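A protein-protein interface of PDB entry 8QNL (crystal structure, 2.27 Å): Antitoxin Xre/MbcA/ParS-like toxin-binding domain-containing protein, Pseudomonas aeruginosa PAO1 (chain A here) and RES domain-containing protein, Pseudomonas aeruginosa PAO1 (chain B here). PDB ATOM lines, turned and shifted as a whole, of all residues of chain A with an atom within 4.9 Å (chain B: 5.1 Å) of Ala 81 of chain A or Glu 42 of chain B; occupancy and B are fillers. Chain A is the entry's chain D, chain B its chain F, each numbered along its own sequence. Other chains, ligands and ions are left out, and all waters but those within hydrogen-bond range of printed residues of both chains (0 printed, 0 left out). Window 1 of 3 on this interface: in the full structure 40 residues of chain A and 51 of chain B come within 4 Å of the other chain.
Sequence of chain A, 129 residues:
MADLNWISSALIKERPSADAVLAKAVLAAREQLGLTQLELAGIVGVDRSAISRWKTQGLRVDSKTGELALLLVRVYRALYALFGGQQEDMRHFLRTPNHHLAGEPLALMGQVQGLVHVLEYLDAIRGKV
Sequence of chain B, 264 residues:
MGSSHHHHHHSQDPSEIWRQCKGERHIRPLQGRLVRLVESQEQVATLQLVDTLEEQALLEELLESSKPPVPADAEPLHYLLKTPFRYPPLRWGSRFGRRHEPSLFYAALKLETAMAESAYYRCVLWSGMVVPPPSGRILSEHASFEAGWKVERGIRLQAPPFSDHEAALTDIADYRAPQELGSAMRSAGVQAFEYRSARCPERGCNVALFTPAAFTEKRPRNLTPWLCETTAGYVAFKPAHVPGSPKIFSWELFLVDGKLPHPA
Arg 77 of chain A touches Glu 42 of chain B (NH2 to CB, 3.7 Å). CD of Arg 77 of chain A touches CG2 of Thr 46 of chain B, at 3.6 Å. Gln 41 of chain B touches Tyr 80 of chain A (O to CD1, 3.8 Å). Ala 45 of chain B touches Tyr 80 of chain A (CB to CG, 3.5 Å). CB of Ala 81 of chain A touches O of Ser 40 of chain B, 3.3 Å away. Ala 81 of chain A touches Gln 41 of chain B (O to OE1, 3.8 Å). CB of Ala 81 of chain A touches CG of Glu 42 of chain B, at 3.8 Å. CA of Gly 84 of chain A touches OE1 of Gln 41 of chain B, 3.5 Å away. Gly 84 of chain A touches Ser 140 of chain B (CA to CA, 3.9 Å). Glu 39 of chain B touches Arg 126 of chain A (OE1 to C, 3.3 Å).
The backbone NH of Lys 128 of chain A is in hydrogen-bond range of the side-chain carboxylate of Glu 39 of chain B, 3.0 Å away. NZ of Lys 128 of chain A is in salt-bridge range of OE1 of Glu 42 of chain B (3.4 Å). The side-chain carboxylate (OE2) of Glu 42 of chain B lies within salt-bridge range of the guanidinium group (NH1) of Arg 126 of chain A, 2.8 Å away. The guanidinium group (NE) of Arg 77 of chain A lies within salt-bridge range of the side-chain carboxylate (OE2) of Glu 60 of chain B, at 2.9 Å.
OE1 of Gln 41 of chain B sits at hydrogen-bond distance from N of Glu 141 of chain B. O of Gln 43 of chain B sits at hydrogen-bond distance from OG1 of Thr 46 of chain B, 3.1 Å away. OG of Ser 40 of chain B lies within hydrogen-bond range of O of Glu 141 of chain B, at 3.1 Å. The side-chain carboxylate (OE2) of Glu 60 of chain B sits at hydrogen-bond distance from the side-chain hydroxyl (OG1) of Thr 46 of chain B (2.8 Å).
Of the 11 printed residues of chain B, 9 touch a printed residue of chain A. Printed residues of chain B that touch a printed residue of chain A: Glu 39, Ser 40, Gln 41, Glu 42, Val 44, Ala 45, Thr 46, Glu 60 and Ser 140. Hydrophobic or aromatic side chains of chain B that line the printed part of chain A: Val 44 and Ala 45. Among the printed residues, Asp or Glu carboxylates within 4 Å of a Lys or Arg side-chain nitrogen of the other chain: Arg 77 of chain A with Glu 60 of chain B (2.9 Å), Arg 126 of chain A with Glu 42 of chain B (2.8 Å) and Lys 128 of chain A with Glu 42 of chain B (3.4 Å).
Ala 81 of chain A touches three residues of chain B. Phe 83 of chain A touches none of the printed residues of chain B. Of the printed residues of chain A, Glu 39 of chain B touches Arg 126 and Lys 128. Of the printed residues of chain A, Gln 41 of chain B touches Tyr 80, Ala 81 and Gly 84. The nearest printed residue of chain A that does not touch Glu 42 of chain B is Ala 78 of chain A (5.5 Å). The nearest printed residue of chain A that does not touch Ser 140 of chain B is Ala 81 of chain A (4.1 Å).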
ATOM      1  N   ARG A  77       4.183 -16.536  23.936  1.00  0.00           N
ATOM      2  CA  ARG A  77       4.925 -16.168  25.139  1.00  0.00           C
ATOM      3  C   ARG A  77       6.425 -16.329  24.932  1.00  0.00           C
ATOM      4  O   ARG A  77       7.208 -15.428  25.259  1.00  0.00           O
ATOM      5  CB  ARG A  77       4.430 -17.024  26.309  1.00  0.00           C
ATOM      6  CG  ARG A  77       4.995 -16.727  27.682  1.00  0.00           C
ATOM      7  CD  ARG A  77       4.208 -17.526  28.733  1.00  0.00           C
ATOM      8  NE  ARG A  77       4.802 -17.454  30.063  1.00  0.00           N
ATOM      9  CZ  ARG A  77       5.734 -18.290  30.505  1.00  0.00           C
ATOM     10  NH1 ARG A  77       6.184 -19.259  29.716  1.00  0.00           N
ATOM     11  NH2 ARG A  77       6.218 -18.157  31.731  1.00  0.00           N
ATOM     12  N   ALA A  78       6.842 -17.467  24.376  1.00  0.00           N
ATOM     13  CA  ALA A  78       8.265 -17.696  24.148  1.00  0.00           C
ATOM     14  C   ALA A  78       8.804 -16.793  23.044  1.00  0.00           C
ATOM     15  O   ALA A  78       9.939 -16.310  23.132  1.00  0.00           O
ATOM     16  CB  ALA A  78       8.510 -19.168  23.820  1.00  0.00           C
ATOM     17  N   LEU A  79       8.006 -16.548  22.000  1.00  0.00           N
ATOM     18  CA  LEU A  79       8.439 -15.654  20.929  1.00  0.00           C
ATOM     19  C   LEU A  79       8.641 -14.235  21.440  1.00  0.00           C
ATOM     20  O   LEU A  79       9.592 -13.550  21.039  1.00  0.00           O
ATOM     21  CB  LEU A  79       7.423 -15.658  19.789  1.00  0.00           C
ATOM     22  CG  LEU A  79       7.532 -16.780  18.763  1.00  0.00           C
ATOM     23  CD1 LEU A  79       6.477 -16.598  17.684  1.00  0.00           C
ATOM     24  CD2 LEU A  79       8.921 -16.783  18.162  1.00  0.00           C
ATOM     25  N   TYR A  80       7.742 -13.769  22.310  1.00  0.00           N
ATOM     26  CA  TYR A  80       7.895 -12.443  22.899  1.00  0.00           C
ATOM     27  C   TYR A  80       9.209 -12.335  23.664  1.00  0.00           C
ATOM     28  O   TYR A  80       9.976 -11.385  23.468  1.00  0.00           O
ATOM     29  CB  TYR A  80       6.701 -12.145  23.812  1.00  0.00           C
ATOM     30  CG  TYR A  80       6.571 -10.701  24.264  1.00  0.00           C
ATOM     31  CD1 TYR A  80       7.390 -10.184  25.265  1.00  0.00           C
ATOM     32  CD2 TYR A  80       5.614  -9.863  23.709  1.00  0.00           C
ATOM     33  CE1 TYR A  80       7.270  -8.872  25.682  1.00  0.00           C
ATOM     34  CE2 TYR A  80       5.485  -8.546  24.123  1.00  0.00           C
ATOM     35  CZ  TYR A  80       6.316  -8.057  25.109  1.00  0.00           C
ATOM     36  OH  TYR A  80       6.187  -6.746  25.518  1.00  0.00           O
ATOM     37  N   ALA A  81       9.498 -13.318  24.518  1.00  0.00           N
ATOM     38  CA  ALA A  81      10.718 -13.275  25.316  1.00  0.00           C
ATOM     39  C   ALA A  81      11.966 -13.381  24.444  1.00  0.00           C
ATOM     40  O   ALA A  81      12.966 -12.703  24.706  1.00  0.00           O
ATOM     41  CB  ALA A  81      10.697 -14.387  26.365  1.00  0.00           C
ATOM     42  N   LEU A  82      11.928 -14.216  23.399  1.00  0.00           N
ATOM     43  CA  LEU A  82      13.102 -14.404  22.547  1.00  0.00           C
ATOM     44  C   LEU A  82      13.379 -13.189  21.670  1.00  0.00           C
ATOM     45  O   LEU A  82      14.542 -12.905  21.355  1.00  0.00           O
ATOM     46  CB  LEU A  82      12.928 -15.639  21.664  1.00  0.00           C
ATOM     47  CG  LEU A  82      13.032 -16.996  22.358  1.00  0.00           C
ATOM     48  CD1 LEU A  82      12.515 -18.107  21.455  1.00  0.00           C
ATOM     49  CD2 LEU A  82      14.470 -17.260  22.770  1.00  0.00           C
ATOM     50  N   PHE A  83      12.338 -12.479  21.241  1.00  0.00           N
ATOM     51  CA  PHE A  83      12.495 -11.344  20.342  1.00  0.00           C
ATOM     52  C   PHE A  83      12.248 -10.010  21.038  1.00  0.00           C
ATOM     53  O   PHE A  83      12.033  -8.997  20.366  1.00  0.00           O
ATOM     54  CB  PHE A  83      11.572 -11.493  19.130  1.00  0.00           C
ATOM     55  CG  PHE A  83      11.988 -12.580  18.176  1.00  0.00           C
ATOM     56  CD1 PHE A  83      12.889 -12.314  17.155  1.00  0.00           C
ATOM     57  CD2 PHE A  83      11.473 -13.858  18.290  1.00  0.00           C
ATOM     58  CE1 PHE A  83      13.272 -13.308  16.272  1.00  0.00           C
ATOM     59  CE2 PHE A  83      11.851 -14.857  17.409  1.00  0.00           C
ATOM     60  CZ  PHE A  83      12.752 -14.581  16.400  1.00  0.00           C
ATOM     61  N   GLY A  84      12.274  -9.990  22.370  1.00  0.00           N
ATOM     62  CA  GLY A  84      12.128  -8.746  23.110  1.00  0.00           C
ATOM     63  C   GLY A  84      10.851  -7.986  22.831  1.00  0.00           C
ATOM     64  O   GLY A  84      10.851  -6.751  22.870  1.00  0.00           O
ATOM     65  N   ARG A 126      15.387 -21.167  24.527  1.00  0.00           N
ATOM     66  CA  ARG A 126      15.465 -20.178  25.592  1.00  0.00           C
ATOM     67  C   ARG A 126      16.536 -20.596  26.589  1.00  0.00           C
ATOM     68  O   ARG A 126      16.615 -21.767  26.974  1.00  0.00           O
ATOM     69  CB  ARG A 126      14.121 -20.017  26.299  1.00  0.00           C
ATOM     70  CG  ARG A 126      13.091 -19.217  25.526  1.00  0.00           C
ATOM     71  CD  ARG A 126      11.898 -18.914  26.409  1.00  0.00           C
ATOM     72  NE  ARG A 126      11.159 -20.128  26.744  1.00  0.00           N
ATOM     73  CZ  ARG A 126      10.424 -20.282  27.841  1.00  0.00           C
ATOM     74  NH1 ARG A 126      10.339 -19.305  28.732  1.00  0.00           N
ATOM     75  NH2 ARG A 126       9.784 -21.423  28.054  1.00  0.00           N
ATOM     76  N   LYS A 128      16.365 -20.072  29.509  1.00  0.00           N
ATOM     77  CA  LYS A 128      15.619 -20.607  30.643  1.00  0.00           C
ATOM     78  C   LYS A 128      15.549 -22.125  30.595  1.00  0.00           C
ATOM     79  O   LYS A 128      15.451 -22.771  31.646  1.00  0.00           O
ATOM     80  CB  LYS A 128      14.205 -20.019  30.670  1.00  0.00           C
ATOM     81  CG  LYS A 128      13.365 -20.436  31.870  1.00  0.00           C
ATOM     82  CD  LYS A 128      13.253 -19.308  32.885  1.00  0.00           C
ATOM     83  CE  LYS A 128      12.645 -18.071  32.239  1.00  0.00           C
ATOM     84  NZ  LYS A 128      12.483 -16.951  33.201  1.00  0.00           N
ATOM     85  N   GLU B  39      16.398 -15.859  29.889  1.00  0.00           N
ATOM     86  CA  GLU B  39      15.529 -14.796  29.418  1.00  0.00           C
ATOM     87  C   GLU B  39      14.524 -14.413  30.494  1.00  0.00           C
ATOM     88  O   GLU B  39      14.152 -15.218  31.350  1.00  0.00           O
ATOM     89  CB  GLU B  39      14.782 -15.207  28.149  1.00  0.00           C
ATOM     90  CG  GLU B  39      15.667 -15.439  26.942  1.00  0.00           C
ATOM     91  CD  GLU B  39      16.313 -16.810  26.947  1.00  0.00           C
ATOM     92  OE1 GLU B  39      16.014 -17.613  27.858  1.00  0.00           O
ATOM     93  OE2 GLU B  39      17.121 -17.089  26.036  1.00  0.00           O
ATOM     94  N   SER B  40      14.102 -13.153  30.455  1.00  0.00           N
ATOM     95  CA  SER B  40      12.960 -12.658  31.204  1.00  0.00           C
ATOM     96  C   SER B  40      11.855 -12.311  30.206  1.00  0.00           C
ATOM     97  O   SER B  40      11.824 -12.883  29.102  1.00  0.00           O
ATOM     98  CB  SER B  40      13.414 -11.490  32.087  1.00  0.00           C
ATOM     99  OG  SER B  40      14.217 -10.577  31.362  1.00  0.00           O
ATOM    100  N   GLN B  41      10.960 -11.398  30.583  1.00  0.00           N
ATOM    101  CA  GLN B  41       9.884 -10.897  29.734  1.00  0.00           C
ATOM    102  C   GLN B  41       8.812 -11.938  29.420  1.00  0.00           C
ATOM    103  O   GLN B  41       7.849 -11.613  28.718  1.00  0.00           O
ATOM    104  CB  GLN B  41      10.401 -10.315  28.409  1.00  0.00           C
ATOM    105  CG  GLN B  41      11.408  -9.184  28.567  1.00  0.00           C
ATOM    106  CD  GLN B  41      11.912  -8.672  27.225  1.00  0.00           C
ATOM    107  OE1 GLN B  41      12.650  -9.364  26.518  1.00  0.00           O
ATOM    108  NE2 GLN B  41      11.518  -7.452  26.872  1.00  0.00           N
ATOM    109  N   GLU B  42       8.942 -13.176  29.899  1.00  0.00           N
ATOM    110  CA  GLU B  42       7.861 -14.146  29.739  1.00  0.00           C
ATOM    111  C   GLU B  42       6.594 -13.684  30.449  1.00  0.00           C
ATOM    112  O   GLU B  42       5.493 -13.784  29.894  1.00  0.00           O
ATOM    113  CB  GLU B  42       8.279 -15.524  30.264  1.00  0.00           C
ATOM    114  CG  GLU B  42       9.235 -16.268  29.361  1.00  0.00           C
ATOM    115  CD  GLU B  42      10.673 -16.116  29.802  1.00  0.00           C
ATOM    116  OE1 GLU B  42      10.930 -15.271  30.688  1.00  0.00           O
ATOM    117  OE2 GLU B  42      11.540 -16.842  29.267  1.00  0.00           O
ATOM    118  N   GLN B  43       6.725 -13.180  31.680  1.00  0.00           N
ATOM    119  CA  GLN B  43       5.551 -12.696  32.397  1.00  0.00           C
ATOM    120  C   GLN B  43       5.042 -11.388  31.811  1.00  0.00           C
ATOM    121  O   GLN B  43       3.830 -11.142  31.810  1.00  0.00           O
ATOM    122  CB  GLN B  43       5.870 -12.525  33.884  1.00  0.00           C
ATOM    123  CG  GLN B  43       6.260 -13.814  34.579  1.00  0.00           C
ATOM    124  CD  GLN B  43       5.300 -14.196  35.688  1.00  0.00           C
ATOM    125  OE1 GLN B  43       4.096 -14.325  35.470  1.00  0.00           O
ATOM    126  NE2 GLN B  43       5.832 -14.376  36.887  1.00  0.00           N
ATOM    127  N   VAL B  44       5.950 -10.536  31.326  1.00  0.00           N
ATOM    128  CA  VAL B  44       5.537  -9.330  30.619  1.00  0.00           C
ATOM    129  C   VAL B  44       4.736  -9.694  29.379  1.00  0.00           C
ATOM    130  O   VAL B  44       3.762  -9.013  29.037  1.00  0.00           O
ATOM    131  CB  VAL B  44       6.773  -8.476  30.271  1.00  0.00           C
ATOM    132  CG1 VAL B  44       6.375  -7.253  29.462  1.00  0.00           C
ATOM    133  CG2 VAL B  44       7.506  -8.066  31.538  1.00  0.00           C
ATOM    134  N   ALA B  45       5.116 -10.781  28.700  1.00  0.00           N
ATOM    135  CA  ALA B  45       4.413 -11.196  27.490  1.00  0.00           C
ATOM    136  C   ALA B  45       2.938 -11.470  27.769  1.00  0.00           C
ATOM    137  O   ALA B  45       2.057 -10.949  27.077  1.00  0.00           O
ATOM    138  CB  ALA B  45       5.083 -12.434  26.897  1.00  0.00           C
ATOM    139  N   THR B  46       2.647 -12.295  28.778  1.00  0.00           N
ATOM    140  CA  THR B  46       1.255 -12.628  29.056  1.00  0.00           C
ATOM    141  C   THR B  46       0.479 -11.451  29.633  1.00  0.00           C
ATOM    142  O   THR B  46      -0.749 -11.411  29.499  1.00  0.00           O
ATOM    143  CB  THR B  46       1.172 -13.824  30.003  1.00  0.00           C
ATOM    144  OG1 THR B  46       2.044 -13.610  31.117  1.00  0.00           O
ATOM    145  CG2 THR B  46       1.587 -15.094  29.274  1.00  0.00           C
ATOM    146  N   GLU B  60      -1.203 -17.473  33.765  1.00  0.00           N
ATOM    147  CA  GLU B  60       0.048 -18.193  33.990  1.00  0.00           C
ATOM    148  C   GLU B  60      -0.190 -19.533  34.680  1.00  0.00           C
ATOM    149  O   GLU B  60       0.561 -20.488  34.445  1.00  0.00           O
ATOM    150  CB  GLU B  60       1.014 -17.325  34.797  1.00  0.00           C
ATOM    151  CG  GLU B  60       1.700 -16.222  33.975  1.00  0.00           C
ATOM    152  CD  GLU B  60       2.766 -16.768  33.034  1.00  0.00           C
ATOM    153  OE1 GLU B  60       3.346 -17.827  33.344  1.00  0.00           O
ATOM    154  OE2 GLU B  60       3.023 -16.136  31.985  1.00  0.00           O
ATOM    155  N   SER B 140      16.485  -7.605  23.466  1.00  0.00           N
ATOM    156  CA  SER B 140      15.815  -8.451  24.439  1.00  0.00           C
ATOM    157  C   SER B 140      16.390  -8.201  25.827  1.00  0.00           C
ATOM    158  O   SER B 140      17.458  -7.601  25.986  1.00  0.00           O
ATOM    159  CB  SER B 140      15.954  -9.938  24.073  1.00  0.00           C
ATOM    160  OG  SER B 140      17.317 -10.319  23.987  1.00  0.00           O
ATOM    161  N   GLU B 141      15.661  -8.669  26.837  1.00  0.00           N
ATOM    162  CA  GLU B 141      16.057  -8.530  28.231  1.00  0.00           C
ATOM    163  C   GLU B 141      16.356  -9.905  28.806  1.00  0.00           C
ATOM    164  O   GLU B 141      15.585 -10.850  28.604  1.00  0.00           O
ATOM    165  CB  GLU B 141      14.969  -7.830  29.050  1.00  0.00           C
ATOM    166  CG  GLU B 141      14.636  -6.434  28.549  1.00  0.00           C
ATOM    167  CD  GLU B 141      13.567  -5.743  29.376  1.00  0.00           C
ATOM    168  OE1 GLU B 141      13.277  -6.208  30.499  1.00  0.00           O
ATOM    169  OE2 GLU B 141      13.014  -4.731  28.896  1.00  0.00           O
